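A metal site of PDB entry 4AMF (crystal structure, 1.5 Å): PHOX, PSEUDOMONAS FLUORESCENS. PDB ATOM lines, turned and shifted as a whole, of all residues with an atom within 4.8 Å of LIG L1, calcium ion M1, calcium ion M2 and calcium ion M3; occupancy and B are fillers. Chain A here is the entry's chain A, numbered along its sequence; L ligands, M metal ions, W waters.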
ATOM      1  N   ASP A  65     -10.289 -31.848  -8.994  1.00  0.00           N
ATOM      2  CA  ASP A  65     -11.091 -30.666  -8.685  1.00  0.00           C
ATOM      3  C   ASP A  65     -10.285 -29.386  -8.953  1.00  0.00           C
ATOM      4  O   ASP A  65      -9.784 -29.248 -10.052  1.00  0.00           O
ATOM      5  CB  ASP A  65     -11.637 -30.856  -7.257  1.00  0.00           C
ATOM      6  CG  ASP A  65     -12.848 -30.076  -6.851  1.00  0.00           C
ATOM      7  OD1 ASP A  65     -13.144 -29.069  -7.489  1.00  0.00           O
ATOM      8  OD2 ASP A  65     -13.560 -30.541  -5.931  1.00  0.00           O
ATOM      9  N   GLU A  86     -10.301 -34.610  -4.735  1.00  0.00           N
ATOM     10  CA  GLU A  86     -11.206 -34.336  -3.611  1.00  0.00           C
ATOM     11  C   GLU A  86     -11.711 -35.520  -2.842  1.00  0.00           C
ATOM     12  O   GLU A  86     -11.752 -35.472  -1.605  1.00  0.00           O
ATOM     13  CB  GLU A  86     -12.388 -33.461  -4.116  1.00  0.00           C
ATOM     14  CG  GLU A  86     -13.217 -32.911  -2.951  1.00  0.00           C
ATOM     15  CD  GLU A  86     -14.479 -32.170  -3.305  1.00  0.00           C
ATOM     16  OE1 GLU A  86     -15.181 -32.608  -4.241  1.00  0.00           O
ATOM     17  OE2 GLU A  86     -14.694 -31.091  -2.735  1.00  0.00           O
ATOM     18  N   CYS A 175     -10.643 -29.634  -2.091  1.00  0.00           N
ATOM     19  CA  CYS A 175     -11.681 -29.137  -2.954  1.00  0.00           C
ATOM     20  C   CYS A 175     -11.121 -28.217  -4.003  1.00  0.00           C
ATOM     21  O   CYS A 175     -10.671 -28.654  -5.088  1.00  0.00           O
ATOM     22  CB  CYS A 175     -12.741 -28.486  -2.085  1.00  0.00           C
ATOM     23  SG  CYS A 175     -14.065 -27.716  -2.986  1.00  0.00           S
ATOM     24  N   GLU A 190     -12.139 -29.125   2.516  1.00  0.00           N
ATOM     25  CA  GLU A 190     -13.549 -28.768   2.596  1.00  0.00           C
ATOM     26  C   GLU A 190     -14.328 -29.742   3.464  1.00  0.00           C
ATOM     27  O   GLU A 190     -14.389 -29.551   4.694  1.00  0.00           O
ATOM     28  CB  GLU A 190     -14.138 -28.624   1.203  1.00  0.00           C
ATOM     29  CG  GLU A 190     -15.568 -28.115   1.179  1.00  0.00           C
ATOM     30  CD  GLU A 190     -16.257 -28.368  -0.141  1.00  0.00           C
ATOM     31  OE1 GLU A 190     -15.857 -29.325  -0.850  1.00  0.00           O
ATOM     32  OE2 GLU A 190     -17.161 -27.583  -0.508  1.00  0.00           O
ATOM     33  N   ASN A 191     -14.921 -30.810   2.904  1.00  0.00           N
ATOM     34  CA  ASN A 191     -15.778 -31.708   3.698  1.00  0.00           C
ATOM     35  C   ASN A 191     -14.988 -32.765   4.479  1.00  0.00           C
ATOM     36  O   ASN A 191     -15.329 -33.945   4.487  1.00  0.00           O
ATOM     37  CB  ASN A 191     -16.860 -32.312   2.810  1.00  0.00           C
ATOM     38  CG  ASN A 191     -17.885 -31.246   2.439  1.00  0.00           C
ATOM     39  OD1 ASN A 191     -18.429 -30.583   3.321  1.00  0.00           O
ATOM     40  ND2 ASN A 191     -18.084 -30.983   1.152  1.00  0.00           N
ATOM     41  N   ARG A 219     -19.934 -39.708   7.340  1.00  0.00           N
ATOM     42  CA  ARG A 219     -20.869 -39.419   6.272  1.00  0.00           C
ATOM     43  C   ARG A 219     -20.604 -40.389   5.131  1.00  0.00           C
ATOM     44  O   ARG A 219     -20.105 -39.995   4.065  1.00  0.00           O
ATOM     45  CB  ARG A 219     -20.800 -37.945   5.832  1.00  0.00           C
ATOM     46  CG  ARG A 219     -21.998 -37.528   4.968  1.00  0.00           C
ATOM     47  CD  ARG A 219     -22.063 -36.042   4.790  1.00  0.00           C
ATOM     48  NE  ARG A 219     -22.391 -35.347   6.034  1.00  0.00           N
ATOM     49  CZ  ARG A 219     -22.248 -34.039   6.242  1.00  0.00           C
ATOM     50  NH1 ARG A 219     -21.770 -33.250   5.289  1.00  0.00           N
ATOM     51  NH2 ARG A 219     -22.557 -33.509   7.415  1.00  0.00           N
ATOM     52  N   GLU A 269     -13.482 -23.931   0.535  1.00  0.00           N
ATOM     53  CA  GLU A 269     -13.661 -24.249  -0.875  1.00  0.00           C
ATOM     54  C   GLU A 269     -12.421 -23.841  -1.682  1.00  0.00           C
ATOM     55  O   GLU A 269     -11.705 -24.702  -2.138  1.00  0.00           O
ATOM     56  CB  GLU A 269     -14.907 -23.582  -1.457  1.00  0.00           C
ATOM     57  CG  GLU A 269     -15.139 -23.954  -2.917  1.00  0.00           C
ATOM     58  CD  GLU A 269     -16.158 -25.017  -3.172  1.00  0.00           C
ATOM     59  OE1 GLU A 269     -16.892 -25.382  -2.234  1.00  0.00           O
ATOM     60  OE2 GLU A 269     -16.163 -25.542  -4.315  1.00  0.00           O
ATOM     61  N   ASP A 288     -17.974 -23.745   2.620  1.00  0.00           N
ATOM     62  CA  ASP A 288     -19.086 -24.304   1.882  1.00  0.00           C
ATOM     63  C   ASP A 288     -19.984 -25.222   2.695  1.00  0.00           C
ATOM     64  O   ASP A 288     -19.893 -26.447   2.668  1.00  0.00           O
ATOM     65  CB  ASP A 288     -18.659 -24.962   0.595  1.00  0.00           C
ATOM     66  CG  ASP A 288     -19.864 -25.437  -0.201  1.00  0.00           C
ATOM     67  OD1 ASP A 288     -20.987 -25.002   0.116  1.00  0.00           O
ATOM     68  OD2 ASP A 288     -19.701 -26.255  -1.086  1.00  0.00           O
ATOM     69  N   GLU A 289     -20.913 -24.586   3.334  1.00  0.00           N
ATOM     70  CA  GLU A 289     -21.986 -25.268   4.075  1.00  0.00           C
ATOM     71  C   GLU A 289     -23.198 -24.330   4.142  1.00  0.00           C
ATOM     72  O   GLU A 289     -23.047 -23.124   4.323  1.00  0.00           O
ATOM     73  CB  GLU A 289     -21.540 -25.749   5.453  1.00  0.00           C
ATOM     74  CG  GLU A 289     -22.603 -26.579   6.166  1.00  0.00           C
ATOM     75  CD  GLU A 289     -22.125 -27.291   7.407  1.00  0.00           C
ATOM     76  OE1 GLU A 289     -20.906 -27.587   7.487  1.00  0.00           O
ATOM     77  OE2 GLU A 289     -22.960 -27.575   8.299  1.00  0.00           O
ATOM     78  N   ARG A 290     -24.389 -24.874   3.937  1.00  0.00           N
ATOM     79  CA  ARG A 290     -25.590 -24.045   4.041  1.00  0.00           C
ATOM     80  C   ARG A 290     -25.578 -23.178   5.324  1.00  0.00           C
ATOM     81  O   ARG A 290     -25.411 -23.690   6.430  1.00  0.00           O
ATOM     82  CB  ARG A 290     -26.859 -24.912   4.087  1.00  0.00           C
ATOM     83  CG  ARG A 290     -27.258 -25.562   2.778  1.00  0.00           C
ATOM     84  CD  ARG A 290     -28.553 -26.332   2.952  1.00  0.00           C
ATOM     85  NE  ARG A 290     -28.334 -27.633   3.563  1.00  0.00           N
ATOM     86  CZ  ARG A 290     -28.043 -28.748   2.897  1.00  0.00           C
ATOM     87  NH1 ARG A 290     -27.931 -28.739   1.563  1.00  0.00           N
ATOM     88  NH2 ARG A 290     -27.852 -29.883   3.535  1.00  0.00           N
ATOM     89  N   ARG A 381     -24.261 -21.170   0.824  1.00  0.00           N
ATOM     90  CA  ARG A 381     -23.170 -22.029   0.366  1.00  0.00           C
ATOM     91  C   ARG A 381     -22.127 -21.374  -0.527  1.00  0.00           C
ATOM     92  O   ARG A 381     -22.097 -21.586  -1.741  1.00  0.00           O
ATOM     93  CB  ARG A 381     -23.729 -23.260  -0.332  1.00  0.00           C
ATOM     94  CG  ARG A 381     -24.435 -24.218   0.610  1.00  0.00           C
ATOM     95  CD  ARG A 381     -24.757 -25.474  -0.126  1.00  0.00           C
ATOM     96  NE  ARG A 381     -23.518 -26.136  -0.537  1.00  0.00           N
ATOM     97  CZ  ARG A 381     -23.418 -27.069  -1.477  1.00  0.00           C
ATOM     98  NH1 ARG A 381     -24.505 -27.516  -2.100  1.00  0.00           N
ATOM     99  NH2 ARG A 381     -22.235 -27.577  -1.794  1.00  0.00           N
ATOM    100  N   GLU A 383     -19.059 -21.085  -2.587  1.00  0.00           N
ATOM    101  CA  GLU A 383     -18.104 -21.991  -3.191  1.00  0.00           C
ATOM    102  C   GLU A 383     -16.934 -21.144  -3.724  1.00  0.00           C
ATOM    103  O   GLU A 383     -16.312 -20.469  -2.897  1.00  0.00           O
ATOM    104  CB  GLU A 383     -18.750 -22.996  -4.149  1.00  0.00           C
ATOM    105  CG  GLU A 383     -19.591 -24.011  -3.380  1.00  0.00           C
ATOM    106  CD  GLU A 383     -19.866 -25.319  -4.104  1.00  0.00           C
ATOM    107  OE1 GLU A 383     -20.785 -25.311  -4.951  1.00  0.00           O
ATOM    108  OE2 GLU A 383     -19.146 -26.325  -3.914  1.00  0.00           O
ATOM    109  N   TRP A 384     -16.585 -21.169  -4.999  1.00  0.00           N
ATOM    110  CA  TRP A 384     -15.377 -20.486  -5.436  1.00  0.00           C
ATOM    111  C   TRP A 384     -15.518 -18.987  -5.416  1.00  0.00           C
ATOM    112  O   TRP A 384     -16.558 -18.440  -5.797  1.00  0.00           O
ATOM    113  CB  TRP A 384     -14.938 -20.922  -6.831  1.00  0.00           C
ATOM    114  CG  TRP A 384     -14.469 -22.327  -6.936  1.00  0.00           C
ATOM    115  CD1 TRP A 384     -15.088 -23.428  -6.445  1.00  0.00           C
ATOM    116  CD2 TRP A 384     -13.489 -22.806  -7.867  1.00  0.00           C
ATOM    117  NE1 TRP A 384     -14.480 -24.562  -6.901  1.00  0.00           N
ATOM    118  CE2 TRP A 384     -13.568 -24.225  -7.858  1.00  0.00           C
ATOM    119  CE3 TRP A 384     -12.556 -22.186  -8.715  1.00  0.00           C
ATOM    120  CZ2 TRP A 384     -12.753 -25.011  -8.652  1.00  0.00           C
ATOM    121  CZ3 TRP A 384     -11.844 -22.978  -9.585  1.00  0.00           C
ATOM    122  CH2 TRP A 384     -11.890 -24.371  -9.502  1.00  0.00           C
ATOM    123  N   THR A 399     -23.901 -21.462  -4.249  1.00  0.00           N
ATOM    124  CA  THR A 399     -24.362 -22.558  -5.111  1.00  0.00           C
ATOM    125  C   THR A 399     -25.805 -22.933  -5.005  1.00  0.00           C
ATOM    126  O   THR A 399     -26.443 -23.168  -6.034  1.00  0.00           O
ATOM    127  CB  THR A 399     -23.423 -23.759  -5.048  1.00  0.00           C
ATOM    128  OG1 THR A 399     -23.600 -24.538  -6.252  1.00  0.00           O
ATOM    129  CG2 THR A 399     -23.600 -24.566  -3.826  1.00  0.00           C
ATOM    130  N   ASP A 475     -20.553 -23.329  -9.179  1.00  0.00           N
ATOM    131  CA  ASP A 475     -19.626 -23.786  -8.156  1.00  0.00           C
ATOM    132  C   ASP A 475     -18.284 -23.158  -8.473  1.00  0.00           C
ATOM    133  O   ASP A 475     -17.936 -22.122  -7.867  1.00  0.00           O
ATOM    134  CB  ASP A 475     -19.695 -25.310  -8.121  1.00  0.00           C
ATOM    135  CG  ASP A 475     -18.738 -25.993  -7.165  1.00  0.00           C
ATOM    136  OD1 ASP A 475     -17.702 -25.410  -6.850  1.00  0.00           O
ATOM    137  OD2 ASP A 475     -19.051 -27.121  -6.724  1.00  0.00           O
ATOM    138  N   ASP A 490     -21.972 -27.472 -10.836  1.00  0.00           N
ATOM    139  CA  ASP A 490     -22.092 -28.674 -10.057  1.00  0.00           C
ATOM    140  C   ASP A 490     -23.499 -28.746  -9.533  1.00  0.00           C
ATOM    141  O   ASP A 490     -23.739 -28.651  -8.332  1.00  0.00           O
ATOM    142  CB  ASP A 490     -21.078 -28.688  -8.893  1.00  0.00           C
ATOM    143  CG  ASP A 490     -21.263 -29.873  -7.962  1.00  0.00           C
ATOM    144  OD1 ASP A 490     -21.776 -30.929  -8.417  1.00  0.00           O
ATOM    145  OD2 ASP A 490     -20.895 -29.749  -6.765  1.00  0.00           O
ATOM    146  N   GLU A 528     -19.602 -33.480 -12.592  1.00  0.00           N
ATOM    147  CA  GLU A 528     -19.618 -32.061 -12.385  1.00  0.00           C
ATOM    148  C   GLU A 528     -18.396 -31.508 -13.154  1.00  0.00           C
ATOM    149  O   GLU A 528     -17.433 -32.259 -13.395  1.00  0.00           O
ATOM    150  CB  GLU A 528     -19.667 -31.607 -10.941  1.00  0.00           C
ATOM    151  CG  GLU A 528     -18.415 -31.868 -10.134  1.00  0.00           C
ATOM    152  CD  GLU A 528     -18.660 -31.617  -8.667  1.00  0.00           C
ATOM    153  OE1 GLU A 528     -19.313 -32.484  -8.047  1.00  0.00           O
ATOM    154  OE2 GLU A 528     -18.264 -30.543  -8.152  1.00  0.00           O
ATOM    155  N   THR A 530     -15.417 -29.004 -12.937  1.00  0.00           N
ATOM    156  CA  THR A 530     -14.690 -28.326 -11.846  1.00  0.00           C
ATOM    157  C   THR A 530     -13.201 -28.272 -12.146  1.00  0.00           C
ATOM    158  O   THR A 530     -12.678 -29.148 -12.835  1.00  0.00           O
ATOM    159  CB  THR A 530     -15.041 -28.985 -10.493  1.00  0.00           C
ATOM    160  OG1 THR A 530     -14.447 -28.230  -9.445  1.00  0.00           O
ATOM    161  CG2 THR A 530     -14.626 -30.426 -10.406  1.00  0.00           C
ATOM    162  N   GLN A 546     -15.227 -34.253 -13.093  1.00  0.00           N
ATOM    163  CA  GLN A 546     -15.191 -34.968 -11.828  1.00  0.00           C
ATOM    164  C   GLN A 546     -16.335 -35.950 -11.700  1.00  0.00           C
ATOM    165  O   GLN A 546     -17.476 -35.630 -12.038  1.00  0.00           O
ATOM    166  CB  GLN A 546     -15.197 -33.960 -10.676  1.00  0.00           C
ATOM    167  CG  GLN A 546     -14.768 -34.528  -9.348  1.00  0.00           C
ATOM    168  CD  GLN A 546     -15.156 -33.664  -8.171  1.00  0.00           C
ATOM    169  OE1 GLN A 546     -16.298 -33.234  -8.065  1.00  0.00           O
ATOM    170  NE2 GLN A 546     -14.216 -33.378  -7.266  1.00  0.00           N
ATOM    171  N   HIS A 547     -16.029 -37.134 -11.204  1.00  0.00           N
ATOM    172  CA  HIS A 547     -16.944 -38.236 -10.991  1.00  0.00           C
ATOM    173  C   HIS A 547     -17.928 -38.507 -12.138  1.00  0.00           C
ATOM    174  O   HIS A 547     -19.118 -38.669 -11.904  1.00  0.00           O
ATOM    175  CB  HIS A 547     -17.673 -38.095  -9.645  1.00  0.00           C
ATOM    176  CG  HIS A 547     -18.537 -36.871  -9.496  1.00  0.00           C
ATOM    177  ND1 HIS A 547     -19.727 -36.739 -10.173  1.00  0.00           N
ATOM    178  CD2 HIS A 547     -18.342 -35.763  -8.754  1.00  0.00           C
ATOM    179  CE1 HIS A 547     -20.240 -35.575  -9.819  1.00  0.00           C
ATOM    180  NE2 HIS A 547     -19.441 -34.939  -8.960  1.00  0.00           N
HETATM  181  P1  LIG L   1     -19.124 -29.963  -3.019  1.00  0.00           P
HETATM  182  O1  LIG L   1     -19.170 -29.740  -4.595  1.00  0.00           O
HETATM  183  O2  LIG L   1     -17.680 -30.653  -2.636  1.00  0.00           O
HETATM  184  O3  LIG L   1     -19.417 -28.634  -2.251  1.00  0.00           O
HETATM  185  P2  LIG L   1     -21.863 -30.816  -3.517  1.00  0.00           P
HETATM  186  O4  LIG L   1     -22.124 -29.385  -3.780  1.00  0.00           O
HETATM  187  O5  LIG L   1     -21.778 -31.827  -4.683  1.00  0.00           O
HETATM  188  C1  LIG L   1     -20.451 -31.027  -2.509  1.00  0.00           C
HETATM  189  P3  LIG L   1     -24.046 -32.404  -2.428  1.00  0.00           P
HETATM  190  O6  LIG L   1     -23.269 -33.641  -2.233  1.00  0.00           O
HETATM  191  O7  LIG L   1     -25.205 -32.337  -3.365  1.00  0.00           O
HETATM  192  O8  LIG L   1     -23.123 -31.176  -2.650  1.00  0.00           O
HETATM  193  O9  LIG L   1     -24.761 -32.006  -0.984  1.00  0.00           O
HETATM  194  C2  LIG L   1     -25.311 -30.698  -0.756  1.00  0.00           C
HETATM  195  C3  LIG L   1     -24.715 -30.069   0.478  1.00  0.00           C
HETATM  196  O10 LIG L   1     -25.193 -30.778   1.637  1.00  0.00           O
HETATM  197  C4  LIG L   1     -23.195 -30.023   0.617  1.00  0.00           C
HETATM  198  O11 LIG L   1     -22.800 -28.794   1.240  1.00  0.00           O
HETATM  199  C5  LIG L   1     -22.891 -31.265   1.455  1.00  0.00           C
HETATM  200  O12 LIG L   1     -21.667 -31.115   2.160  1.00  0.00           O
HETATM  201  C6  LIG L   1     -24.118 -31.324   2.382  1.00  0.00           C
HETATM  202  N1  LIG L   1     -24.497 -32.655   2.815  1.00  0.00           N
HETATM  203  C7  LIG L   1     -24.435 -33.824   2.104  1.00  0.00           C
HETATM  204  N2  LIG L   1     -24.860 -34.881   2.764  1.00  0.00           N
HETATM  205  C8  LIG L   1     -25.232 -34.371   3.995  1.00  0.00           C
HETATM  206  C9  LIG L   1     -25.711 -34.988   5.175  1.00  0.00           C
HETATM  207  N3  LIG L   1     -25.831 -36.303   5.329  1.00  0.00           N
HETATM  208  N4  LIG L   1     -25.982 -34.181   6.228  1.00  0.00           N
HETATM  209  C10 LIG L   1     -25.757 -32.871   6.122  1.00  0.00           C
HETATM  210  N5  LIG L   1     -25.291 -32.191   5.063  1.00  0.00           N
HETATM  211  C11 LIG L   1     -25.034 -32.994   4.036  1.00  0.00           C
HETATM  212 FE1  LG2 L   2     -15.926 -29.499  -2.946  1.00  0.00          FE
HETATM  213 FE2  LG2 L   2     -18.124 -27.041  -2.224  1.00  0.00          FE
HETATM  214  O1  LG2 L   2     -17.021 -28.016  -3.511  1.00  0.00           O
HETATM  215 CA    CA M   1     -20.660 -27.954  -5.198  1.00  0.00          CA
HETATM  216 CA    CA M   2     -16.938 -27.276  -5.610  1.00  0.00          CA
HETATM  217 CA    CA M   3     -19.649 -31.563  -5.945  1.00  0.00          CA
HETATM  218  O   HOH W   1     -25.136 -34.399  -5.308  1.00  0.00           O
HETATM  219  O   HOH W   2     -14.374 -27.314  -6.057  1.00  0.00           O
HETATM  220  O   HOH W   3     -24.998 -28.661  -4.725  1.00  0.00           O
HETATM  221  O   HOH W   4     -24.469 -27.632   3.175  1.00  0.00           O
HETATM  222  O   HOH W   5     -17.290 -32.088  -5.685  1.00  0.00           O
HETATM  223  O   HOH W   6     -20.708 -33.806   2.697  1.00  0.00           O
HETATM  224  O   HOH W   7     -20.544 -28.945   3.786  1.00  0.00           O
HETATM  225  O   HOH W   8     -21.260 -34.892  -3.112  1.00  0.00           O
HETATM  226  O   HOH W   9     -20.112 -28.635   0.521  1.00  0.00           O
HETATM  227  O   HOH W  10     -23.624 -32.096  -6.566  1.00  0.00           O
HETATM  228  O   HOH W  11     -24.768 -29.407   5.309  1.00  0.00           O
HETATM  229  O   HOH W  12     -17.238 -32.681  -0.975  1.00  0.00           O
HETATM  230  O   HOH W  13     -15.923 -29.728  -5.271  1.00  0.00           O
HETATM  231  O   HOH W  14     -16.713 -28.317  -7.831  1.00  0.00           O
HETATM  232  O   HOH W  15     -22.650 -27.165  -6.063  1.00  0.00           O
HETATM  233  O   HOH W  16     -19.831 -33.961  -5.245  1.00  0.00           O
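Water W15 lies within hydrogen-bond range of the side-chain hydroxyl of Thr 399 (2.8 Å) and the backbone carbonyl oxygen of Asp 490 (2.9 Å).
Water W2 lies within hydrogen-bond range of the side-chain carboxylate of Asp 65 (2.6 Å) and the indole nitrogen of Trp 384 (2.9 Å).
Water W9 lies within hydrogen-bond range of an oxygen (O11) of LIG L1 (2.8 Å), the backbone carbonyl oxygen (O) of Asp 288 (3.1 Å), the side-chain amide nitrogen (ND2) of Asn 191 (3.2 Å) and the guanidinium group (NH2) of Arg 381 (3.3 Å).
Water W4 bridges O11 of LIG L1 (2.8 Å) and N of Arg 290 (2.9 Å).
Water W6 lies within hydrogen-bond range of the guanidinium group of Arg 219 (2.9 Å) and an oxygen (O12) of LIG L1 (2.9 Å).
Water W7 lies within hydrogen-bond range of the side-chain amide oxygen of Asn 191 (2.7 Å), the backbone carbonyl oxygen of Asp 288 (2.8 Å) and an oxygen (O12) of LIG L1 (2.9 Å).
Two residues have an atom within 4 Å of calcium ion M3: Asp 490 and Glu 528.
O1 of LIG L1 is bound to calcium ion M3 (2.3 Å).
OE1 of Glu 528 binds calcium ion M3, 2.3 Å away.
OD2 of Asp 490 binds calcium ion M3.
Water W5 binds calcium ion M3, 2.4 Å away.
O5 of LIG L1 is bound to calcium ion M3 (2.5 Å).
Water W16 binds calcium ion M3 (2.5 Å).
The side-chain carboxylate (OE2) of Glu 528 binds calcium ion M3 (2.8 Å).
Calcium ion M2 is bound by an oxygen (O1) of LG2 L2 (2.2 Å), the side-chain carboxylate (OE2) of Glu 269 (2.3 Å), the side-chain carboxylate (OD1) of Asp 475 (2.4 Å), the side-chain carboxylate (OD2) of Asp 475 (2.4 Å), water W14 (2.5 Å), water W2 (2.6 Å) and water W13 (2.7 Å).
Calcium ion M2 has seven donor atoms within binding distance.
Slightly farther from calcium ion M2 lies the side-chain carboxylate (OE2) of Glu 383 (2.9 Å).
Calcium ion M1 is bound by water W15 (2.3 Å), the side-chain carboxylate (OD2) of Asp 475 (2.4 Å), the side-chain carboxylate (OD2) of Asp 490 (2.4 Å), an oxygen (O1) of LIG L1 (2.4 Å), an oxygen (O4) of LIG L1 (2.5 Å), the side-chain carboxylate (OE2) of Glu 383 (2.6 Å) and the side-chain carboxylate (OE1) of Glu 383 (2.7 Å).
FE2 of LG2 L2 is bound by OE2 of Glu 383 (2.1 Å).
The side-chain amide oxygen (OD1) of Asn 191 lies within hydrogen-bond range of an oxygen (O12) of LIG L1.
The guanidinium group (NE) of Arg 381 is in hydrogen-bond range of an oxygen (O11) of LIG L1, 3.3 Å away.
FE2 of LG2 L2 is bound by OD2 of Asp 288, 2.1 Å away.
The side-chain carboxylate (OE2) of Glu 86 binds an iron atom (FE1) of LG2 L2 (2.0 Å).
An iron atom (FE2) of LG2 L2 is bound by the side-chain carboxylate (OE2) of Glu 190, at 2.0 Å.
OE1 of Glu 269 binds FE2 of LG2 L2 (2.1 Å).
The side-chain sulfur (SG) of Cys 175 binds an iron atom (FE1) of LG2 L2 (2.6 Å).
The guanidinium group (NH2) of Arg 290 lies within hydrogen-bond range of an oxygen (O10) of LIG L1, at 3.4 Å.
OE2 of Glu 86 lies close to O2 of LIG L1 (3.0 Å).
OE1 of Glu 190 lies close to O2 of LIG L1, 2.9 Å away.
The side-chain carboxylate (OD2) of Asp 288 lies close to an oxygen (O3) of LIG L1.
Merely in contact with LIG L1: Arg 219.
11 residues have an atom within 4 Å of LIG L1: Glu 86, Glu 190, Asn 191, Arg 219, Asp 288, Arg 290, Arg 381, Glu 383, Asp 475, Asp 490 and Glu 528.
The side-chain carboxylate (OE1) of Glu 86 is in hydrogen-bond range of the side-chain amide nitrogen (NE2) of Gln 546, 3.3 Å away.
The side-chain carboxylate (OE1) of Glu 383 lies close to the side-chain hydroxyl (OG1) of Thr 399 (3.2 Å).
The backbone NH of Thr 399 lies within hydrogen-bond range of the backbone carbonyl oxygen of Arg 381, 3.1 Å away.
The side-chain carboxylate of Glu 383 lies close to the guanidinium group of Arg 381, at 3.95 Å.
O of Asp 475 lies within hydrogen-bond range of N of Trp 384 (3.3 Å).
A ring nitrogen (NE2) of His 547 sits close to the side-chain carboxylate (OE1) of Glu 528, 2.6 Å away.
OE1 of Glu 190 sits close to ND2 of Asn 191 (3.4 Å).
The guanidinium group (NE) of Arg 381 is in salt-bridge range of the side-chain carboxylate (OD1) of Asp 288.
Residues that only touch calcium ion M2: Cys 175 and Trp 384.
An oxygen (O3) of LIG L1 binds an iron atom (FE2) of LG2 L2, at 2.1 Å.
Arg 381 touches calcium ion M1.
Four residues have an atom within 4 Å of calcium ion M1: Arg 381, Glu 383, Asp 475 and Asp 490.
Along chain A the residues within 4 Å of calcium ion M1 span positions 381 to 490.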
